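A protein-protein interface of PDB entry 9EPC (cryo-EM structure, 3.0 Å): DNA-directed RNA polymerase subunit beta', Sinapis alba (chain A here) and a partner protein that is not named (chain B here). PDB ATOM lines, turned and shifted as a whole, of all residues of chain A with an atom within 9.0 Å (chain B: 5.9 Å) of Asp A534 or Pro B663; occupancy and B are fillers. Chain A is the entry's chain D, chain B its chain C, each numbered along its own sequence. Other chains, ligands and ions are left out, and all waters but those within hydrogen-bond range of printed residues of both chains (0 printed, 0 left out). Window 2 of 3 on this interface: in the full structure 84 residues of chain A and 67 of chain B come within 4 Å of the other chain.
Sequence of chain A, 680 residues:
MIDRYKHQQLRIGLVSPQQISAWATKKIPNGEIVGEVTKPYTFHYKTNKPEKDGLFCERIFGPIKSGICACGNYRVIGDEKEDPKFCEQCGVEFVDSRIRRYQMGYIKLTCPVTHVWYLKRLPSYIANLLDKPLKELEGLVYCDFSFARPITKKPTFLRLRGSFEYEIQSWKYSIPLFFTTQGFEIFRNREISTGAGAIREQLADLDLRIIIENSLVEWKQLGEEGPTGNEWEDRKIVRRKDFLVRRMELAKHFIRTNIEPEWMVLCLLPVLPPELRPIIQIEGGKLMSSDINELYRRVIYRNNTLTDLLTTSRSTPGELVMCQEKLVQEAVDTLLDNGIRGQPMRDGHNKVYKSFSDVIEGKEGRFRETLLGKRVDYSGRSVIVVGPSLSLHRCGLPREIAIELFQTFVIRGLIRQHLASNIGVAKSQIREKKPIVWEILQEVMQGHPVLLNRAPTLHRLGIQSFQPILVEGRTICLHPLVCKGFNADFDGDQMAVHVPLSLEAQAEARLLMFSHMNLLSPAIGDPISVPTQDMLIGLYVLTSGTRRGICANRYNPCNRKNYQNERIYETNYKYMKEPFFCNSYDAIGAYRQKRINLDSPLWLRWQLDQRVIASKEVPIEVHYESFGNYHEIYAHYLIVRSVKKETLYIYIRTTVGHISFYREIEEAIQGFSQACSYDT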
ATOM      1  N   VAL A 386       2.497 -30.720 -30.094  1.00  0.00           N
ATOM      2  CA  VAL A 386       1.546 -29.644 -29.834  1.00  0.00           C
ATOM      3  C   VAL A 386       0.890 -29.240 -31.145  1.00  0.00           C
ATOM      4  O   VAL A 386       1.574 -28.878 -32.107  1.00  0.00           O
ATOM      5  CB  VAL A 386       2.237 -28.443 -29.175  1.00  0.00           C
ATOM      6  CG1 VAL A 386       1.250 -27.669 -28.316  1.00  0.00           C
ATOM      7  CG2 VAL A 386       3.424 -28.902 -28.363  1.00  0.00           C
ATOM      8  N   PRO A 388      -1.060 -26.389 -31.841  1.00  0.00           N
ATOM      9  CA  PRO A 388      -1.599 -25.114 -31.339  1.00  0.00           C
ATOM     10  C   PRO A 388      -2.729 -24.554 -32.181  1.00  0.00           C
ATOM     11  O   PRO A 388      -3.525 -23.758 -31.670  1.00  0.00           O
ATOM     12  CB  PRO A 388      -0.378 -24.191 -31.359  1.00  0.00           C
ATOM     13  CG  PRO A 388       0.432 -24.707 -32.472  1.00  0.00           C
ATOM     14  CD  PRO A 388       0.254 -26.201 -32.476  1.00  0.00           C
ATOM     15  N   PRO A 480      -2.987 -27.582 -27.175  1.00  0.00           N
ATOM     16  CA  PRO A 480      -2.157 -27.136 -26.042  1.00  0.00           C
ATOM     17  C   PRO A 480      -2.904 -27.082 -24.720  1.00  0.00           C
ATOM     18  O   PRO A 480      -2.317 -27.380 -23.673  1.00  0.00           O
ATOM     19  CB  PRO A 480      -1.686 -25.746 -26.488  1.00  0.00           C
ATOM     20  CG  PRO A 480      -2.715 -25.298 -27.467  1.00  0.00           C
ATOM     21  CD  PRO A 480      -3.129 -26.534 -28.199  1.00  0.00           C
ATOM     22  N   LYS A 484      -2.502 -29.848 -20.732  1.00  0.00           N
ATOM     23  CA  LYS A 484      -2.404 -29.601 -19.299  1.00  0.00           C
ATOM     24  C   LYS A 484      -3.355 -30.489 -18.508  1.00  0.00           C
ATOM     25  O   LYS A 484      -3.024 -30.913 -17.395  1.00  0.00           O
ATOM     26  CB  LYS A 484      -2.681 -28.127 -18.996  1.00  0.00           C
ATOM     27  CG  LYS A 484      -1.622 -27.179 -19.533  1.00  0.00           C
ATOM     28  CD  LYS A 484      -0.263 -27.466 -18.917  1.00  0.00           C
ATOM     29  CE  LYS A 484      -0.289 -27.275 -17.408  1.00  0.00           C
ATOM     30  NZ  LYS A 484       1.014 -27.621 -16.779  1.00  0.00           N
ATOM     31  N   PHE A 490       6.152 -32.027 -23.144  1.00  0.00           N
ATOM     32  CA  PHE A 490       6.659 -32.242 -24.493  1.00  0.00           C
ATOM     33  C   PHE A 490       8.156 -32.527 -24.479  1.00  0.00           C
ATOM     34  O   PHE A 490       8.866 -32.234 -25.441  1.00  0.00           O
ATOM     35  CB  PHE A 490       6.317 -31.054 -25.385  1.00  0.00           C
ATOM     36  CG  PHE A 490       4.854 -30.735 -25.402  1.00  0.00           C
ATOM     37  CD1 PHE A 490       3.950 -31.612 -25.976  1.00  0.00           C
ATOM     38  CD2 PHE A 490       4.376 -29.577 -24.819  1.00  0.00           C
ATOM     39  CE1 PHE A 490       2.599 -31.331 -25.980  1.00  0.00           C
ATOM     40  CE2 PHE A 490       3.028 -29.291 -24.821  1.00  0.00           C
ATOM     41  CZ  PHE A 490       2.140 -30.167 -25.402  1.00  0.00           C
ATOM     42  N   PRO A 531      -6.067 -20.750 -19.594  1.00  0.00           N
ATOM     43  CA  PRO A 531      -4.821 -20.486 -20.321  1.00  0.00           C
ATOM     44  C   PRO A 531      -3.630 -20.451 -19.376  1.00  0.00           C
ATOM     45  O   PRO A 531      -3.700 -19.902 -18.276  1.00  0.00           O
ATOM     46  CB  PRO A 531      -5.071 -19.119 -20.964  1.00  0.00           C
ATOM     47  CG  PRO A 531      -6.548 -19.035 -21.088  1.00  0.00           C
ATOM     48  CD  PRO A 531      -7.101 -19.747 -19.890  1.00  0.00           C
ATOM     49  N   THR A 532      -2.529 -21.051 -19.818  1.00  0.00           N
ATOM     50  CA  THR A 532      -1.311 -21.129 -19.029  1.00  0.00           C
ATOM     51  C   THR A 532      -0.114 -20.937 -19.948  1.00  0.00           C
ATOM     52  O   THR A 532      -0.247 -20.875 -21.173  1.00  0.00           O
ATOM     53  CB  THR A 532      -1.195 -22.466 -18.286  1.00  0.00           C
ATOM     54  OG1 THR A 532      -1.414 -23.546 -19.201  1.00  0.00           O
ATOM     55  CG2 THR A 532      -2.206 -22.549 -17.152  1.00  0.00           C
ATOM     56  N   GLN A 533       1.060 -20.842 -19.338  1.00  0.00           N
ATOM     57  CA  GLN A 533       2.344 -20.747 -20.051  1.00  0.00           C
ATOM     58  C   GLN A 533       2.307 -19.480 -20.910  1.00  0.00           C
ATOM     59  O   GLN A 533       1.832 -18.433 -20.446  1.00  0.00           O
ATOM     60  CB  GLN A 533       2.600 -22.025 -20.811  1.00  0.00           C
ATOM     61  CG  GLN A 533       2.469 -23.283 -19.980  1.00  0.00           C
ATOM     62  CD  GLN A 533       3.687 -23.544 -19.127  1.00  0.00           C
ATOM     63  OE1 GLN A 533       4.684 -22.832 -19.215  1.00  0.00           O
ATOM     64  NE2 GLN A 533       3.614 -24.576 -18.296  1.00  0.00           N
ATOM     65  N   ASP A 534       2.783 -19.538 -22.156  1.00  0.00           N
ATOM     66  CA  ASP A 534       2.861 -18.341 -22.983  1.00  0.00           C
ATOM     67  C   ASP A 534       1.491 -17.817 -23.389  1.00  0.00           C
ATOM     68  O   ASP A 534       1.384 -16.652 -23.781  1.00  0.00           O
ATOM     69  CB  ASP A 534       3.712 -18.606 -24.224  1.00  0.00           C
ATOM     70  CG  ASP A 534       3.549 -20.012 -24.752  1.00  0.00           C
ATOM     71  OD1 ASP A 534       3.012 -20.866 -24.016  1.00  0.00           O
ATOM     72  OD2 ASP A 534       3.963 -20.265 -25.902  1.00  0.00           O
ATOM     73  N   MET A 535       0.446 -18.642 -23.314  1.00  0.00           N
ATOM     74  CA  MET A 535      -0.901 -18.117 -23.500  1.00  0.00           C
ATOM     75  C   MET A 535      -1.224 -17.079 -22.440  1.00  0.00           C
ATOM     76  O   MET A 535      -1.790 -16.024 -22.740  1.00  0.00           O
ATOM     77  CB  MET A 535      -1.918 -19.254 -23.459  1.00  0.00           C
ATOM     78  CG  MET A 535      -1.742 -20.253 -24.570  1.00  0.00           C
ATOM     79  SD  MET A 535      -2.104 -21.940 -24.064  1.00  0.00           S
ATOM     80  CE  MET A 535      -3.839 -21.776 -23.690  1.00  0.00           C
ATOM     81  N   LEU A 536      -0.858 -17.358 -21.190  1.00  0.00           N
ATOM     82  CA  LEU A 536      -1.087 -16.401 -20.118  1.00  0.00           C
ATOM     83  C   LEU A 536      -0.127 -15.223 -20.202  1.00  0.00           C
ATOM     84  O   LEU A 536      -0.479 -14.108 -19.800  1.00  0.00           O
ATOM     85  CB  LEU A 536      -0.959 -17.104 -18.772  1.00  0.00           C
ATOM     86  CG  LEU A 536      -1.379 -16.328 -17.533  1.00  0.00           C
ATOM     87  CD1 LEU A 536      -2.809 -15.854 -17.675  1.00  0.00           C
ATOM     88  CD2 LEU A 536      -1.227 -17.222 -16.325  1.00  0.00           C
ATOM     89  N   ILE A 537       1.088 -15.448 -20.707  1.00  0.00           N
ATOM     90  CA  ILE A 537       2.039 -14.354 -20.876  1.00  0.00           C
ATOM     91  C   ILE A 537       1.522 -13.350 -21.895  1.00  0.00           C
ATOM     92  O   ILE A 537       1.568 -12.136 -21.670  1.00  0.00           O
ATOM     93  CB  ILE A 537       3.422 -14.904 -21.273  1.00  0.00           C
ATOM     94  CG1 ILE A 537       4.258 -15.192 -20.029  1.00  0.00           C
ATOM     95  CG2 ILE A 537       4.154 -13.924 -22.167  1.00  0.00           C
ATOM     96  CD1 ILE A 537       4.574 -13.960 -19.218  1.00  0.00           C
ATOM     97  N   GLY A 538       1.012 -13.840 -23.026  1.00  0.00           N
ATOM     98  CA  GLY A 538       0.538 -12.936 -24.059  1.00  0.00           C
ATOM     99  C   GLY A 538      -0.620 -12.077 -23.594  1.00  0.00           C
ATOM    100  O   GLY A 538      -0.675 -10.881 -23.888  1.00  0.00           O
ATOM    101  N   LEU A 539      -1.558 -12.674 -22.862  1.00  0.00           N
ATOM    102  CA  LEU A 539      -2.671 -11.904 -22.322  1.00  0.00           C
ATOM    103  C   LEU A 539      -2.194 -10.908 -21.278  1.00  0.00           C
ATOM    104  O   LEU A 539      -2.713  -9.789 -21.195  1.00  0.00           O
ATOM    105  CB  LEU A 539      -3.711 -12.844 -21.726  1.00  0.00           C
ATOM    106  CG  LEU A 539      -4.235 -13.932 -22.655  1.00  0.00           C
ATOM    107  CD1 LEU A 539      -5.098 -14.889 -21.867  1.00  0.00           C
ATOM    108  CD2 LEU A 539      -5.011 -13.322 -23.806  1.00  0.00           C
ATOM    109  N   TYR A 540      -1.214 -11.301 -20.463  1.00  0.00           N
ATOM    110  CA  TYR A 540      -0.684 -10.392 -19.455  1.00  0.00           C
ATOM    111  C   TYR A 540      -0.042  -9.172 -20.099  1.00  0.00           C
ATOM    112  O   TYR A 540      -0.202  -8.048 -19.613  1.00  0.00           O
ATOM    113  CB  TYR A 540       0.320 -11.123 -18.567  1.00  0.00           C
ATOM    114  CG  TYR A 540       0.898 -10.257 -17.477  1.00  0.00           C
ATOM    115  CD1 TYR A 540       0.185 -10.003 -16.316  1.00  0.00           C
ATOM    116  CD2 TYR A 540       2.158  -9.691 -17.610  1.00  0.00           C
ATOM    117  CE1 TYR A 540       0.708  -9.211 -15.318  1.00  0.00           C
ATOM    118  CE2 TYR A 540       2.688  -8.897 -16.617  1.00  0.00           C
ATOM    119  CZ  TYR A 540       1.959  -8.660 -15.474  1.00  0.00           C
ATOM    120  OH  TYR A 540       2.483  -7.870 -14.480  1.00  0.00           O
ATOM    121  N   VAL A 541       0.695  -9.376 -21.192  1.00  0.00           N
ATOM    122  CA  VAL A 541       1.318  -8.255 -21.888  1.00  0.00           C
ATOM    123  C   VAL A 541       0.259  -7.334 -22.478  1.00  0.00           C
ATOM    124  O   VAL A 541       0.381  -6.105 -22.418  1.00  0.00           O
ATOM    125  CB  VAL A 541       2.286  -8.767 -22.968  1.00  0.00           C
ATOM    126  CG1 VAL A 541       2.838  -7.602 -23.755  1.00  0.00           C
ATOM    127  CG2 VAL A 541       3.410  -9.557 -22.332  1.00  0.00           C
ATOM    128  N   TYR B 661      15.368 -17.713 -28.096  1.00  0.00           N
ATOM    129  CA  TYR B 661      14.522 -18.101 -26.971  1.00  0.00           C
ATOM    130  C   TYR B 661      13.319 -17.167 -26.933  1.00  0.00           C
ATOM    131  O   TYR B 661      13.279 -16.189 -26.192  1.00  0.00           O
ATOM    132  CB  TYR B 661      15.303 -18.058 -25.664  1.00  0.00           C
ATOM    133  CG  TYR B 661      16.250 -19.212 -25.464  1.00  0.00           C
ATOM    134  CD1 TYR B 661      17.514 -19.203 -26.031  1.00  0.00           C
ATOM    135  CD2 TYR B 661      15.886 -20.305 -24.697  1.00  0.00           C
ATOM    136  CE1 TYR B 661      18.381 -20.251 -25.847  1.00  0.00           C
ATOM    137  CE2 TYR B 661      16.747 -21.358 -24.507  1.00  0.00           C
ATOM    138  CZ  TYR B 661      17.993 -21.327 -25.084  1.00  0.00           C
ATOM    139  OH  TYR B 661      18.858 -22.378 -24.898  1.00  0.00           O
ATOM    140  N   MET B 662      12.324 -17.480 -27.751  1.00  0.00           N
ATOM    141  CA  MET B 662      11.094 -16.709 -27.774  1.00  0.00           C
ATOM    142  C   MET B 662       9.916 -17.645 -27.988  1.00  0.00           C
ATOM    143  O   MET B 662      10.066 -18.701 -28.611  1.00  0.00           O
ATOM    144  CB  MET B 662      11.114 -15.646 -28.880  1.00  0.00           C
ATOM    145  CG  MET B 662      11.411 -16.192 -30.260  1.00  0.00           C
ATOM    146  SD  MET B 662      11.060 -14.983 -31.543  1.00  0.00           S
ATOM    147  CE  MET B 662       9.335 -14.651 -31.202  1.00  0.00           C
ATOM    148  N   PRO B 663       8.742 -17.296 -27.469  1.00  0.00           N
ATOM    149  CA  PRO B 663       7.539 -18.052 -27.822  1.00  0.00           C
ATOM    150  C   PRO B 663       7.128 -17.746 -29.249  1.00  0.00           C
ATOM    151  O   PRO B 663       7.160 -16.595 -29.689  1.00  0.00           O
ATOM    152  CB  PRO B 663       6.500 -17.555 -26.814  1.00  0.00           C
ATOM    153  CG  PRO B 663       6.965 -16.194 -26.453  1.00  0.00           C
ATOM    154  CD  PRO B 663       8.462 -16.240 -26.483  1.00  0.00           C
ATOM    155  N   TRP B 664       6.751 -18.790 -29.985  1.00  0.00           N
ATOM    156  CA  TRP B 664       6.398 -18.655 -31.397  1.00  0.00           C
ATOM    157  C   TRP B 664       5.073 -19.363 -31.658  1.00  0.00           C
ATOM    158  O   TRP B 664       5.054 -20.545 -32.005  1.00  0.00           O
ATOM    159  CB  TRP B 664       7.503 -19.199 -32.286  1.00  0.00           C
ATOM    160  CG  TRP B 664       7.546 -18.548 -33.626  1.00  0.00           C
ATOM    161  CD1 TRP B 664       8.373 -17.540 -34.016  1.00  0.00           C
ATOM    162  CD2 TRP B 664       6.717 -18.846 -34.753  1.00  0.00           C
ATOM    163  NE1 TRP B 664       8.118 -17.197 -35.319  1.00  0.00           N
ATOM    164  CE2 TRP B 664       7.103 -17.985 -35.794  1.00  0.00           C
ATOM    165  CE3 TRP B 664       5.685 -19.760 -34.984  1.00  0.00           C
ATOM    166  CZ2 TRP B 664       6.500 -18.011 -37.044  1.00  0.00           C
ATOM    167  CZ3 TRP B 664       5.089 -19.784 -36.226  1.00  0.00           C
ATOM    168  CH2 TRP B 664       5.495 -18.915 -37.239  1.00  0.00           C
ATOM    169  N   GLU B 665       3.971 -18.635 -31.483  1.00  0.00           N
ATOM    170  CA  GLU B 665       2.632 -19.076 -31.869  1.00  0.00           C
ATOM    171  C   GLU B 665       2.236 -20.401 -31.231  1.00  0.00           C
ATOM    172  O   GLU B 665       1.335 -21.083 -31.724  1.00  0.00           O
ATOM    173  CB  GLU B 665       2.506 -19.173 -33.392  1.00  0.00           C
ATOM    174  CG  GLU B 665       2.804 -17.877 -34.121  1.00  0.00           C
ATOM    175  CD  GLU B 665       1.724 -16.831 -33.923  1.00  0.00           C
ATOM    176  OE1 GLU B 665       0.622 -17.188 -33.458  1.00  0.00           O
ATOM    177  OE2 GLU B 665       1.977 -15.650 -34.237  1.00  0.00           O
ATOM    178  N   GLY B 666       2.889 -20.786 -30.141  1.00  0.00           N
ATOM    179  CA  GLY B 666       2.560 -22.014 -29.457  1.00  0.00           C
ATOM    180  C   GLY B 666       3.222 -23.258 -29.999  1.00  0.00           C
ATOM    181  O   GLY B 666       3.029 -24.338 -29.428  1.00  0.00           O
ATOM    182  N   ASN B 668       6.308 -23.824 -29.811  1.00  0.00           N
ATOM    183  CA  ASN B 668       7.291 -24.170 -28.792  1.00  0.00           C
ATOM    184  C   ASN B 668       6.668 -24.182 -27.402  1.00  0.00           C
ATOM    185  O   ASN B 668       7.355 -23.913 -26.414  1.00  0.00           O
ATOM    186  CB  ASN B 668       8.486 -23.216 -28.839  1.00  0.00           C
ATOM    187  CG  ASN B 668       8.074 -21.766 -28.808  1.00  0.00           C
ATOM    188  OD1 ASN B 668       6.907 -21.443 -28.601  1.00  0.00           O
ATOM    189  ND2 ASN B 668       9.036 -20.877 -29.009  1.00  0.00           N
ATOM    190  N   PHE B 669       5.372 -24.477 -27.315  1.00  0.00           N
ATOM    191  CA  PHE B 669       4.687 -24.553 -26.033  1.00  0.00           C
ATOM    192  C   PHE B 669       5.350 -25.587 -25.135  1.00  0.00           C
ATOM    193  O   PHE B 669       5.633 -26.710 -25.560  1.00  0.00           O
ATOM    194  CB  PHE B 669       3.218 -24.905 -26.261  1.00  0.00           C
ATOM    195  CG  PHE B 669       2.384 -24.899 -25.016  1.00  0.00           C
ATOM    196  CD1 PHE B 669       1.846 -23.722 -24.536  1.00  0.00           C
ATOM    197  CD2 PHE B 669       2.118 -26.074 -24.342  1.00  0.00           C
ATOM    198  CE1 PHE B 669       1.069 -23.716 -23.401  1.00  0.00           C
ATOM    199  CE2 PHE B 669       1.342 -26.073 -23.203  1.00  0.00           C
ATOM    200  CZ  PHE B 669       0.818 -24.891 -22.732  1.00  0.00           C
ATOM    201  N   GLU B 670       5.593 -25.198 -23.883  1.00  0.00           N
ATOM    202  CA  GLU B 670       6.321 -26.023 -22.926  1.00  0.00           C
ATOM    203  C   GLU B 670       7.668 -26.459 -23.485  1.00  0.00           C
ATOM    204  O   GLU B 670       8.553 -25.626 -23.707  1.00  0.00           O
ATOM    205  CB  GLU B 670       5.497 -27.244 -22.516  1.00  0.00           C
ATOM    206  CG  GLU B 670       4.371 -26.935 -21.552  1.00  0.00           C
ATOM    207  CD  GLU B 670       3.657 -28.182 -21.079  1.00  0.00           C
ATOM    208  OE1 GLU B 670       4.057 -29.289 -21.497  1.00  0.00           O
ATOM    209  OE2 GLU B 670       2.697 -28.059 -20.292  1.00  0.00           O
ATOM    210  N   VAL B 853      13.887 -22.507 -32.371  1.00  0.00           N
ATOM    211  CA  VAL B 853      13.278 -21.545 -31.462  1.00  0.00           C
ATOM    212  C   VAL B 853      12.853 -22.291 -30.207  1.00  0.00           C
ATOM    213  O   VAL B 853      12.088 -23.258 -30.284  1.00  0.00           O
ATOM    214  CB  VAL B 853      12.085 -20.828 -32.108  1.00  0.00           C
ATOM    215  CG1 VAL B 853      11.538 -19.784 -31.172  1.00  0.00           C
ATOM    216  CG2 VAL B 853      12.499 -20.196 -33.417  1.00  0.00           C
ATOM    217  N   PHE B 854      13.348 -21.843 -29.060  1.00  0.00           N
ATOM    218  CA  PHE B 854      13.053 -22.460 -27.778  1.00  0.00           C
ATOM    219  C   PHE B 854      12.082 -21.605 -26.981  1.00  0.00           C
ATOM    220  O   PHE B 854      11.956 -20.399 -27.197  1.00  0.00           O
ATOM    221  CB  PHE B 854      14.326 -22.670 -26.959  1.00  0.00           C
ATOM    222  CG  PHE B 854      15.096 -23.890 -27.338  1.00  0.00           C
ATOM    223  CD1 PHE B 854      14.792 -25.114 -26.778  1.00  0.00           C
ATOM    224  CD2 PHE B 854      16.130 -23.813 -28.245  1.00  0.00           C
ATOM    225  CE1 PHE B 854      15.504 -26.239 -27.120  1.00  0.00           C
ATOM    226  CE2 PHE B 854      16.844 -24.929 -28.589  1.00  0.00           C
ATOM    227  CZ  PHE B 854      16.531 -26.146 -28.027  1.00  0.00           C
ATOM    228  N   ASN B 855      11.405 -22.247 -26.044  1.00  0.00           N
ATOM    229  CA  ASN B 855      10.513 -21.535 -25.146  1.00  0.00           C
ATOM    230  C   ASN B 855      11.323 -20.910 -24.019  1.00  0.00           C
ATOM    231  O   ASN B 855      12.001 -21.636 -23.284  1.00  0.00           O
ATOM    232  CB  ASN B 855       9.468 -22.478 -24.575  1.00  0.00           C
ATOM    233  CG  ASN B 855       8.257 -21.749 -24.039  1.00  0.00           C
ATOM    234  OD1 ASN B 855       8.305 -20.549 -23.785  1.00  0.00           O
ATOM    235  ND2 ASN B 855       7.162 -22.474 -23.864  1.00  0.00           N
ATOM    236  N   PRO B 856      11.299 -19.588 -23.855  1.00  0.00           N
ATOM    237  CA  PRO B 856      12.012 -18.981 -22.725  1.00  0.00           C
ATOM    238  C   PRO B 856      11.442 -19.363 -21.372  1.00  0.00           C
ATOM    239  O   PRO B 856      12.150 -19.233 -20.369  1.00  0.00           O
ATOM    240  CB  PRO B 856      11.865 -17.478 -22.985  1.00  0.00           C
ATOM    241  CG  PRO B 856      10.627 -17.368 -23.795  1.00  0.00           C
ATOM    242  CD  PRO B 856      10.611 -18.580 -24.675  1.00  0.00           C
ATOM    243  N   LEU B 857      10.194 -19.831 -21.310  1.00  0.00           N
ATOM    244  CA  LEU B 857       9.590 -20.185 -20.031  1.00  0.00           C
ATOM    245  C   LEU B 857      10.251 -21.394 -19.388  1.00  0.00           C
ATOM    246  O   LEU B 857      10.065 -21.620 -18.190  1.00  0.00           O
ATOM    247  CB  LEU B 857       8.100 -20.462 -20.206  1.00  0.00           C
ATOM    248  CG  LEU B 857       7.272 -19.403 -20.927  1.00  0.00           C
ATOM    249  CD1 LEU B 857       5.829 -19.843 -20.987  1.00  0.00           C
ATOM    250  CD2 LEU B 857       7.390 -18.071 -20.231  1.00  0.00           C
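Printed residues of chain B within 4 Å of Lys A484: Glu B670 (3.3 Å).
Of chain B, only Pro B663 (3.8 Å), Phe B669 (3.1 Å) and Leu B857 (3.3 Å) come within 4 Å of Asp A534.
Tyr B661 touches none of the printed residues of chain A.
Of chain A, only Asp A534 (3.8 Å) comes within 4 Å of Pro B663.
Printed residues of chain A within 4 Å of Gly B666: Val A386 (3.9 Å) and Pro A388 (3.9 Å).
Printed residues of chain A within 4 Å of Phe B669: Val A386 (3.97 Å), Pro A480 (3.9 Å), Phe A490 (3.2 Å), Thr A532 (3.8 Å), Gln A533 (3.5 Å), Asp A534 (3.1 Å) and Met A535 (3.7 Å).
The nearest residue of chain B that does not touch Asp A534 is Asn B668 (4.2 Å).
The nearest printed residue of chain B that does not touch Met A535 is Leu B857 (6.0 Å).
OE2 of Glu B670 lies within salt-bridge range of NZ of Lys A484, at 3.9 Å.
Hydrophobic or aromatic side chains of chain B that line the printed part of chain A: Pro B663, Phe B669 and Leu B857.
Hydrophobic or aromatic side chains of chain A that line the printed part of chain B: Val A386, Pro A388, Phe A490 and Met A535.
Among the printed residues, merely in contact across the chains: Val A386 with Gly B666, Val A386 with Phe B669, Pro A388 with Glu B665, Pro A388 with Gly B666, Pro A480 with Phe B669, Phe A490 with Phe B669, Phe A490 with Glu B670, Thr A532 with Phe B669, Gln A533 with Phe B669, Gln A533 with Leu B857, Asp A534 with Pro B663, Asp A534 with Phe B669, Asp A534 with Leu B857 and Met A535 with Phe B669.
The side-chain amide nitrogen (ND2) of Asn B855 lies close to the backbone NH (N) of Glu B670, at 3.1 Å.
The backbone NH (N) of Leu B857 lies close to the side-chain amide oxygen (OD1) of Asn B855, at 3.2 Å.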
